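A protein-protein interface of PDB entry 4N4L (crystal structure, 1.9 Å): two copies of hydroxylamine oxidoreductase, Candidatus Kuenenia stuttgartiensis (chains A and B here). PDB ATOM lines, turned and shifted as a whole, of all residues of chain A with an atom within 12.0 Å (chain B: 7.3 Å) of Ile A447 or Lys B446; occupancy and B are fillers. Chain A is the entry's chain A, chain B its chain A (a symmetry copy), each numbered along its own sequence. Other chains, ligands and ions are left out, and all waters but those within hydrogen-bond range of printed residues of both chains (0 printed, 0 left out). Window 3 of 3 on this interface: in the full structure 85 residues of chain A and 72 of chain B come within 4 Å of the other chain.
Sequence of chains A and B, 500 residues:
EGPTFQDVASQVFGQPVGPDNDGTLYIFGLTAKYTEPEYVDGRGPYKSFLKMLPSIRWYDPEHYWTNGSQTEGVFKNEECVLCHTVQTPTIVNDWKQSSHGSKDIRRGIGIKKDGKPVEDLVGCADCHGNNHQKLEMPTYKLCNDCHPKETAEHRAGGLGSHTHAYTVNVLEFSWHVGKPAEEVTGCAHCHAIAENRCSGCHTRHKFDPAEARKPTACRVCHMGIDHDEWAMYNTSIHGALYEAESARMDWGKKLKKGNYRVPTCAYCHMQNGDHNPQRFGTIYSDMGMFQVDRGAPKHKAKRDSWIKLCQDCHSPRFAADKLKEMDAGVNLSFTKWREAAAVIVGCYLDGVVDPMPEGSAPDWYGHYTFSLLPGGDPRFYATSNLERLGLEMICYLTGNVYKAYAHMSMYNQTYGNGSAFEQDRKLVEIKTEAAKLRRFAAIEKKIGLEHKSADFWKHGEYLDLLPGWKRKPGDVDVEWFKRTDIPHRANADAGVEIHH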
ATOM      1  N   ARG A 438      12.351   4.002 -22.991  1.00  0.00           N
ATOM      2  CA  ARG A 438      12.775   3.002 -22.013  1.00  0.00           C
ATOM      3  C   ARG A 438      13.127   3.620 -20.662  1.00  0.00           C
ATOM      4  O   ARG A 438      12.789   3.049 -19.615  1.00  0.00           O
ATOM      5  CB  ARG A 438      13.933   2.167 -22.566  1.00  0.00           C
ATOM      6  CG  ARG A 438      13.462   1.197 -23.633  1.00  0.00           C
ATOM      7  CD  ARG A 438      14.584   0.368 -24.232  1.00  0.00           C
ATOM      8  NE  ARG A 438      14.050  -0.547 -25.239  1.00  0.00           N
ATOM      9  CZ  ARG A 438      13.387  -1.672 -24.966  1.00  0.00           C
ATOM     10  NH1 ARG A 438      13.185  -2.058 -23.705  1.00  0.00           N
ATOM     11  NH2 ARG A 438      12.926  -2.424 -25.957  1.00  0.00           N
ATOM     12  N   ARG A 439      13.777   4.783 -20.675  1.00  0.00           N
ATOM     13  CA  ARG A 439      14.124   5.467 -19.425  1.00  0.00           C
ATOM     14  C   ARG A 439      12.890   5.953 -18.677  1.00  0.00           C
ATOM     15  O   ARG A 439      12.834   5.833 -17.451  1.00  0.00           O
ATOM     16  CB  ARG A 439      15.077   6.636 -19.666  1.00  0.00           C
ATOM     17  CG  ARG A 439      16.474   6.207 -20.019  1.00  0.00           C
ATOM     18  CD  ARG A 439      17.378   7.393 -20.271  1.00  0.00           C
ATOM     19  NE  ARG A 439      18.079   7.850 -19.071  1.00  0.00           N
ATOM     20  CZ  ARG A 439      18.998   8.816 -19.068  1.00  0.00           C
ATOM     21  NH1 ARG A 439      19.321   9.447 -20.196  1.00  0.00           N
ATOM     22  NH2 ARG A 439      19.598   9.163 -17.939  1.00  0.00           N
ATOM     23  N   PHE A 440      11.913   6.502 -19.402  1.00  0.00           N
ATOM     24  CA  PHE A 440      10.639   6.895 -18.788  1.00  0.00           C
ATOM     25  C   PHE A 440       9.942   5.696 -18.149  1.00  0.00           C
ATOM     26  O   PHE A 440       9.486   5.775 -17.008  1.00  0.00           O
ATOM     27  CB  PHE A 440       9.676   7.527 -19.806  1.00  0.00           C
ATOM     28  CG  PHE A 440       9.836   9.017 -19.981  1.00  0.00           C
ATOM     29  CD1 PHE A 440       9.818   9.877 -18.885  1.00  0.00           C
ATOM     30  CD2 PHE A 440       9.941   9.570 -21.254  1.00  0.00           C
ATOM     31  CE1 PHE A 440       9.948  11.252 -19.051  1.00  0.00           C
ATOM     32  CE2 PHE A 440      10.073  10.945 -21.427  1.00  0.00           C
ATOM     33  CZ  PHE A 440      10.073  11.787 -20.324  1.00  0.00           C
ATOM     34  N   ALA A 441       9.854   4.594 -18.892  1.00  0.00           N
ATOM     35  CA  ALA A 441       9.168   3.395 -18.413  1.00  0.00           C
ATOM     36  C   ALA A 441       9.852   2.792 -17.180  1.00  0.00           C
ATOM     37  O   ALA A 441       9.176   2.367 -16.239  1.00  0.00           O
ATOM     38  CB  ALA A 441       9.063   2.359 -19.527  1.00  0.00           C
ATOM     39  N   ALA A 442      11.183   2.770 -17.183  1.00  0.00           N
ATOM     40  CA  ALA A 442      11.956   2.261 -16.048  1.00  0.00           C
ATOM     41  C   ALA A 442      11.737   3.105 -14.788  1.00  0.00           C
ATOM     42  O   ALA A 442      11.570   2.559 -13.691  1.00  0.00           O
ATOM     43  CB  ALA A 442      13.443   2.198 -16.396  1.00  0.00           C
ATOM     44  N   ILE A 443      11.724   4.427 -14.950  1.00  0.00           N
ATOM     45  CA  ILE A 443      11.476   5.344 -13.835  1.00  0.00           C
ATOM     46  C   ILE A 443      10.061   5.162 -13.294  1.00  0.00           C
ATOM     47  O   ILE A 443       9.865   4.993 -12.091  1.00  0.00           O
ATOM     48  CB  ILE A 443      11.678   6.821 -14.251  1.00  0.00           C
ATOM     49  CG1 ILE A 443      13.168   7.121 -14.440  1.00  0.00           C
ATOM     50  CG2 ILE A 443      11.087   7.773 -13.212  1.00  0.00           C
ATOM     51  CD1 ILE A 443      13.443   8.387 -15.225  1.00  0.00           C
ATOM     52  N   GLU A 444       9.083   5.189 -14.192  1.00  0.00           N
ATOM     53  CA  GLU A 444       7.678   5.058 -13.807  1.00  0.00           C
ATOM     54  C   GLU A 444       7.376   3.726 -13.116  1.00  0.00           C
ATOM     55  O   GLU A 444       6.572   3.679 -12.182  1.00  0.00           O
ATOM     56  CB  GLU A 444       6.780   5.258 -15.027  1.00  0.00           C
ATOM     57  CG  GLU A 444       6.773   6.710 -15.512  1.00  0.00           C
ATOM     58  CD  GLU A 444       6.264   6.880 -16.934  1.00  0.00           C
ATOM     59  OE1 GLU A 444       6.183   8.041 -17.385  1.00  0.00           O
ATOM     60  OE2 GLU A 444       5.953   5.866 -17.603  1.00  0.00           O
ATOM     61  N   LYS A 445       8.019   2.652 -13.566  1.00  0.00           N
ATOM     62  CA  LYS A 445       7.884   1.352 -12.907  1.00  0.00           C
ATOM     63  C   LYS A 445       8.430   1.406 -11.477  1.00  0.00           C
ATOM     64  O   LYS A 445       7.758   0.976 -10.544  1.00  0.00           O
ATOM     65  CB  LYS A 445       8.599   0.247 -13.696  1.00  0.00           C
ATOM     66  CG  LYS A 445       8.476  -1.135 -13.043  1.00  0.00           C
ATOM     67  CD  LYS A 445       9.003  -2.257 -13.916  1.00  0.00           C
ATOM     68  CE  LYS A 445       8.895  -3.597 -13.185  1.00  0.00           C
ATOM     69  NZ  LYS A 445       9.678  -4.669 -13.859  1.00  0.00           N
ATOM     70  N   LYS A 446       9.634   1.950 -11.311  1.00  0.00           N
ATOM     71  CA  LYS A 446      10.292   1.984 -10.000  1.00  0.00           C
ATOM     72  C   LYS A 446       9.519   2.799  -8.963  1.00  0.00           C
ATOM     73  O   LYS A 446       9.416   2.388  -7.807  1.00  0.00           O
ATOM     74  CB  LYS A 446      11.724   2.529 -10.109  1.00  0.00           C
ATOM     75  CG  LYS A 446      12.565   2.279  -8.859  1.00  0.00           C
ATOM     76  CD  LYS A 446      13.903   2.988  -8.912  1.00  0.00           C
ATOM     77  CE  LYS A 446      14.643   2.891  -7.571  1.00  0.00           C
ATOM     78  NZ  LYS A 446      14.834   1.487  -7.112  1.00  0.00           N
ATOM     79  N   ILE A 447       8.991   3.950  -9.371  1.00  0.00           N
ATOM     80  CA  ILE A 447       8.247   4.821  -8.452  1.00  0.00           C
ATOM     81  C   ILE A 447       6.749   4.482  -8.375  1.00  0.00           C
ATOM     82  O   ILE A 447       6.023   5.070  -7.574  1.00  0.00           O
ATOM     83  CB  ILE A 447       8.439   6.324  -8.803  1.00  0.00           C
ATOM     84  CG1 ILE A 447       7.672   6.715 -10.077  1.00  0.00           C
ATOM     85  CG2 ILE A 447       9.924   6.647  -8.945  1.00  0.00           C
ATOM     86  CD1 ILE A 447       7.824   8.187 -10.448  1.00  0.00           C
ATOM     87  N   GLY A 448       6.291   3.548  -9.204  1.00  0.00           N
ATOM     88  CA  GLY A 448       4.887   3.130  -9.199  1.00  0.00           C
ATOM     89  C   GLY A 448       3.926   4.157  -9.774  1.00  0.00           C
ATOM     90  O   GLY A 448       2.772   4.242  -9.344  1.00  0.00           O
ATOM     91  N   LEU A 449       4.395   4.941 -10.746  1.00  0.00           N
ATOM     92  CA  LEU A 449       3.536   5.879 -11.460  1.00  0.00           C
ATOM     93  C   LEU A 449       2.896   5.145 -12.637  1.00  0.00           C
ATOM     94  O   LEU A 449       3.596   4.564 -13.465  1.00  0.00           O
ATOM     95  CB  LEU A 449       4.342   7.085 -11.958  1.00  0.00           C
ATOM     96  CG  LEU A 449       3.547   8.266 -12.532  1.00  0.00           C
ATOM     97  CD1 LEU A 449       4.378   9.540 -12.500  1.00  0.00           C
ATOM     98  CD2 LEU A 449       3.064   7.986 -13.957  1.00  0.00           C
ATOM     99  N   GLU A 450       1.568   5.161 -12.694  1.00  0.00           N
ATOM    100  CA  GLU A 450       0.837   4.528 -13.787  1.00  0.00           C
ATOM    101  C   GLU A 450       0.657   5.555 -14.897  1.00  0.00           C
ATOM    102  O   GLU A 450      -0.185   6.449 -14.799  1.00  0.00           O
ATOM    103  CB  GLU A 450      -0.523   4.013 -13.303  1.00  0.00           C
ATOM    104  CG  GLU A 450      -1.270   3.167 -14.340  1.00  0.00           C
ATOM    105  CD  GLU A 450      -2.625   2.677 -13.845  1.00  0.00           C
ATOM    106  OE1 GLU A 450      -3.569   2.610 -14.669  1.00  0.00           O
ATOM    107  OE2 GLU A 450      -2.748   2.354 -12.638  1.00  0.00           O
ATOM    108  N   HIS A 451       1.465   5.437 -15.945  1.00  0.00           N
ATOM    109  CA  HIS A 451       1.420   6.399 -17.042  1.00  0.00           C
ATOM    110  C   HIS A 451       0.243   6.105 -17.962  1.00  0.00           C
ATOM    111  O   HIS A 451       0.027   4.959 -18.355  1.00  0.00           O
ATOM    112  CB  HIS A 451       2.725   6.377 -17.843  1.00  0.00           C
ATOM    113  CG  HIS A 451       2.652   7.142 -19.130  1.00  0.00           C
ATOM    114  ND1 HIS A 451       2.589   8.517 -19.174  1.00  0.00           N
ATOM    115  CD2 HIS A 451       2.612   6.719 -20.417  1.00  0.00           C
ATOM    116  CE1 HIS A 451       2.523   8.911 -20.435  1.00  0.00           C
ATOM    117  NE2 HIS A 451       2.536   7.839 -21.208  1.00  0.00           N
ATOM    118  N   LYS A 452      -0.524   7.143 -18.283  1.00  0.00           N
ATOM    119  CA  LYS A 452      -1.540   7.062 -19.323  1.00  0.00           C
ATOM    120  C   LYS A 452      -1.119   7.981 -20.462  1.00  0.00           C
ATOM    121  O   LYS A 452      -0.831   9.159 -20.240  1.00  0.00           O
ATOM    122  CB  LYS A 452      -2.909   7.490 -18.791  1.00  0.00           C
ATOM    123  CG  LYS A 452      -3.479   6.566 -17.724  1.00  0.00           C
ATOM    124  CD  LYS A 452      -4.788   7.113 -17.170  1.00  0.00           C
ATOM    125  CE  LYS A 452      -5.329   6.234 -16.047  1.00  0.00           C
ATOM    126  NZ  LYS A 452      -5.724   4.878 -16.535  1.00  0.00           N
ATOM    127  N   PHE B 440       7.816  14.048 -17.757  1.00  0.00           N
ATOM    128  CA  PHE B 440       8.816  14.593 -16.831  1.00  0.00           C
ATOM    129  C   PHE B 440       8.148  15.295 -15.651  1.00  0.00           C
ATOM    130  O   PHE B 440       8.517  15.068 -14.500  1.00  0.00           O
ATOM    131  CB  PHE B 440       9.759  15.593 -17.519  1.00  0.00           C
ATOM    132  CG  PHE B 440      10.972  14.971 -18.166  1.00  0.00           C
ATOM    133  CD1 PHE B 440      11.810  14.117 -17.452  1.00  0.00           C
ATOM    134  CD2 PHE B 440      11.314  15.291 -19.476  1.00  0.00           C
ATOM    135  CE1 PHE B 440      12.937  13.559 -18.045  1.00  0.00           C
ATOM    136  CE2 PHE B 440      12.440  14.734 -20.076  1.00  0.00           C
ATOM    137  CZ  PHE B 440      13.254  13.870 -19.359  1.00  0.00           C
ATOM    138  N   ALA B 441       7.175  16.156 -15.946  1.00  0.00           N
ATOM    139  CA  ALA B 441       6.490  16.929 -14.910  1.00  0.00           C
ATOM    140  C   ALA B 441       5.722  16.031 -13.932  1.00  0.00           C
ATOM    141  O   ALA B 441       5.743  16.268 -12.722  1.00  0.00           O
ATOM    142  CB  ALA B 441       5.556  17.956 -15.539  1.00  0.00           C
ATOM    143  N   ALA B 442       5.063  14.999 -14.457  1.00  0.00           N
ATOM    144  CA  ALA B 442       4.327  14.043 -13.626  1.00  0.00           C
ATOM    145  C   ALA B 442       5.260  13.273 -12.685  1.00  0.00           C
ATOM    146  O   ALA B 442       4.941  13.084 -11.505  1.00  0.00           O
ATOM    147  CB  ALA B 442       3.533  13.073 -14.501  1.00  0.00           C
ATOM    148  N   ILE B 443       6.410  12.845 -13.204  1.00  0.00           N
ATOM    149  CA  ILE B 443       7.410  12.140 -12.399  1.00  0.00           C
ATOM    150  C   ILE B 443       7.969  13.055 -11.313  1.00  0.00           C
ATOM    151  O   ILE B 443       8.002  12.690 -10.139  1.00  0.00           O
ATOM    152  CB  ILE B 443       8.574  11.607 -13.268  1.00  0.00           C
ATOM    153  CG1 ILE B 443       8.107  10.416 -14.110  1.00  0.00           C
ATOM    154  CG2 ILE B 443       9.765  11.193 -12.404  1.00  0.00           C
ATOM    155  CD1 ILE B 443       9.025  10.087 -15.269  1.00  0.00           C
ATOM    156  N   GLU B 444       8.399  14.245 -11.717  1.00  0.00           N
ATOM    157  CA  GLU B 444       8.987  15.208 -10.785  1.00  0.00           C
ATOM    158  C   GLU B 444       8.018  15.630  -9.679  1.00  0.00           C
ATOM    159  O   GLU B 444       8.429  15.823  -8.533  1.00  0.00           O
ATOM    160  CB  GLU B 444       9.508  16.425 -11.551  1.00  0.00           C
ATOM    161  CG  GLU B 444      10.745  16.098 -12.389  1.00  0.00           C
ATOM    162  CD  GLU B 444      11.038  17.121 -13.476  1.00  0.00           C
ATOM    163  OE1 GLU B 444      12.059  16.949 -14.173  1.00  0.00           O
ATOM    164  OE2 GLU B 444      10.254  18.084 -13.643  1.00  0.00           O
ATOM    165  N   LYS B 445       6.738  15.765 -10.016  1.00  0.00           N
ATOM    166  CA  LYS B 445       5.714  16.058  -9.012  1.00  0.00           C
ATOM    167  C   LYS B 445       5.600  14.916  -7.998  1.00  0.00           C
ATOM    168  O   LYS B 445       5.614  15.157  -6.794  1.00  0.00           O
ATOM    169  CB  LYS B 445       4.348  16.314  -9.663  1.00  0.00           C
ATOM    170  CG  LYS B 445       3.246  16.633  -8.647  1.00  0.00           C
ATOM    171  CD  LYS B 445       1.949  17.083  -9.293  1.00  0.00           C
ATOM    172  CE  LYS B 445       0.882  17.336  -8.226  1.00  0.00           C
ATOM    173  NZ  LYS B 445      -0.478  17.469  -8.814  1.00  0.00           N
ATOM    174  N   LYS B 446       5.508  13.681  -8.488  1.00  0.00           N
ATOM    175  CA  LYS B 446       5.315  12.516  -7.617  1.00  0.00           C
ATOM    176  C   LYS B 446       6.472  12.299  -6.642  1.00  0.00           C
ATOM    177  O   LYS B 446       6.245  11.979  -5.475  1.00  0.00           O
ATOM    178  CB  LYS B 446       5.096  11.237  -8.437  1.00  0.00           C
ATOM    179  CG  LYS B 446       4.562  10.070  -7.609  1.00  0.00           C
ATOM    180  CD  LYS B 446       4.535   8.772  -8.390  1.00  0.00           C
ATOM    181  CE  LYS B 446       4.189   7.580  -7.488  1.00  0.00           C
ATOM    182  NZ  LYS B 446       2.903   7.756  -6.758  1.00  0.00           N
ATOM    183  N   ILE B 447       7.703  12.461  -7.120  1.00  0.00           N
ATOM    184  CA  ILE B 447       8.888  12.256  -6.277  1.00  0.00           C
ATOM    185  C   ILE B 447       9.317  13.523  -5.518  1.00  0.00           C
ATOM    186  O   ILE B 447      10.236  13.472  -4.702  1.00  0.00           O
ATOM    187  CB  ILE B 447      10.084  11.690  -7.093  1.00  0.00           C
ATOM    188  CG1 ILE B 447      10.704  12.755  -8.012  1.00  0.00           C
ATOM    189  CG2 ILE B 447       9.642  10.470  -7.899  1.00  0.00           C
ATOM    190  CD1 ILE B 447      11.891  12.241  -8.821  1.00  0.00           C
ATOM    191  N   GLY B 448       8.662  14.649  -5.788  1.00  0.00           N
ATOM    192  CA  GLY B 448       8.971  15.907  -5.107  1.00  0.00           C
ATOM    193  C   GLY B 448      10.291  16.537  -5.524  1.00  0.00           C
ATOM    194  O   GLY B 448      10.950  17.198  -4.716  1.00  0.00           O
ATOM    195  N   LEU B 449      10.681  16.336  -6.783  1.00  0.00           N
ATOM    196  CA  LEU B 449      11.864  16.988  -7.336  1.00  0.00           C
ATOM    197  C   LEU B 449      11.446  18.346  -7.895  1.00  0.00           C
ATOM    198  O   LEU B 449      10.542  18.428  -8.726  1.00  0.00           O
ATOM    199  CB  LEU B 449      12.494  16.128  -8.438  1.00  0.00           C
ATOM    200  CG  LEU B 449      13.868  16.567  -8.964  1.00  0.00           C
ATOM    201  CD1 LEU B 449      14.584  15.403  -9.634  1.00  0.00           C
ATOM    202  CD2 LEU B 449      13.754  17.746  -9.933  1.00  0.00           C
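Ala A442 touches none of the printed residues of chain B.
Of the printed residues of chain B, Ile A443 touches Ile B443.
Ile A447 touches just these residues of chain B: Lys B446 and Ile B447.
Of the printed residues of chain A, Phe B440 touches Phe A440.
No residue of chain A comes within 4 Å of Lys B445.
Lys B446 touches just these residues of chain A: Ile A447 and Leu A449.
Ile B447 touches just one residue of chain A: Ile A447 (3.9 Å).
No residue of chain A comes within 4 Å of Gly B448.
The nearest printed residue of chain B that does not touch Leu A449 is Glu B444 (6.2 Å).
Phe A440 touches Ile B443, but with the chains exchanged Ile A443 does not touch Phe B440 (5.9 Å).
Ile A447 touches Lys B446, but with the chains exchanged Lys A446 does not touch Ile B447 (7.7 Å).
Ile B447 touches its own counterpart, Ile A447.
Leu A449 touches Ile B443, but with the chains exchanged Ile A443 does not touch Leu B449 (9.0 Å).
Positions printed for both chains: 440, 441, 442, 443, 444, 445, 446, 447, 448 and 449.
Of the 8 pairs that touch across the chains among the printed residues, 3 have their exchanged pair printed and touching as well.
N of Leu A449 sits at hydrogen-bond distance from O of Glu A444, at 2.9 Å.
Printed residues of chain A that touch a printed residue of chain B: Phe A440, Ile A443, Ile A447 and Leu A449.
Hydrophobic or aromatic side chains of chain A within 4 Å of the printed part of chain B: Phe A440, Ile A443, Ile A447 and Leu A449.
Hydrophobic or aromatic side chains of chain B within 4 Å of the printed part of chain A: Phe B440, Ile B443 and Ile B447.
Among the printed residues, 8 pairs touch across the chains.
Among the printed residues, no Asp or Glu carboxylate lies within 4 Å of a Lys or Arg side-chain nitrogen of the other chain.
Among the printed residues, merely in contact across the chains: Phe A440 with Phe B440, Phe A440 with Ile B443, Ile A443 with Ile B443, Ile A447 with Lys B446, Ile A447 with Ile B447, Leu A449 with Ala B442, Leu A449 with Ile B443 and Leu A449 with Lys B446.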
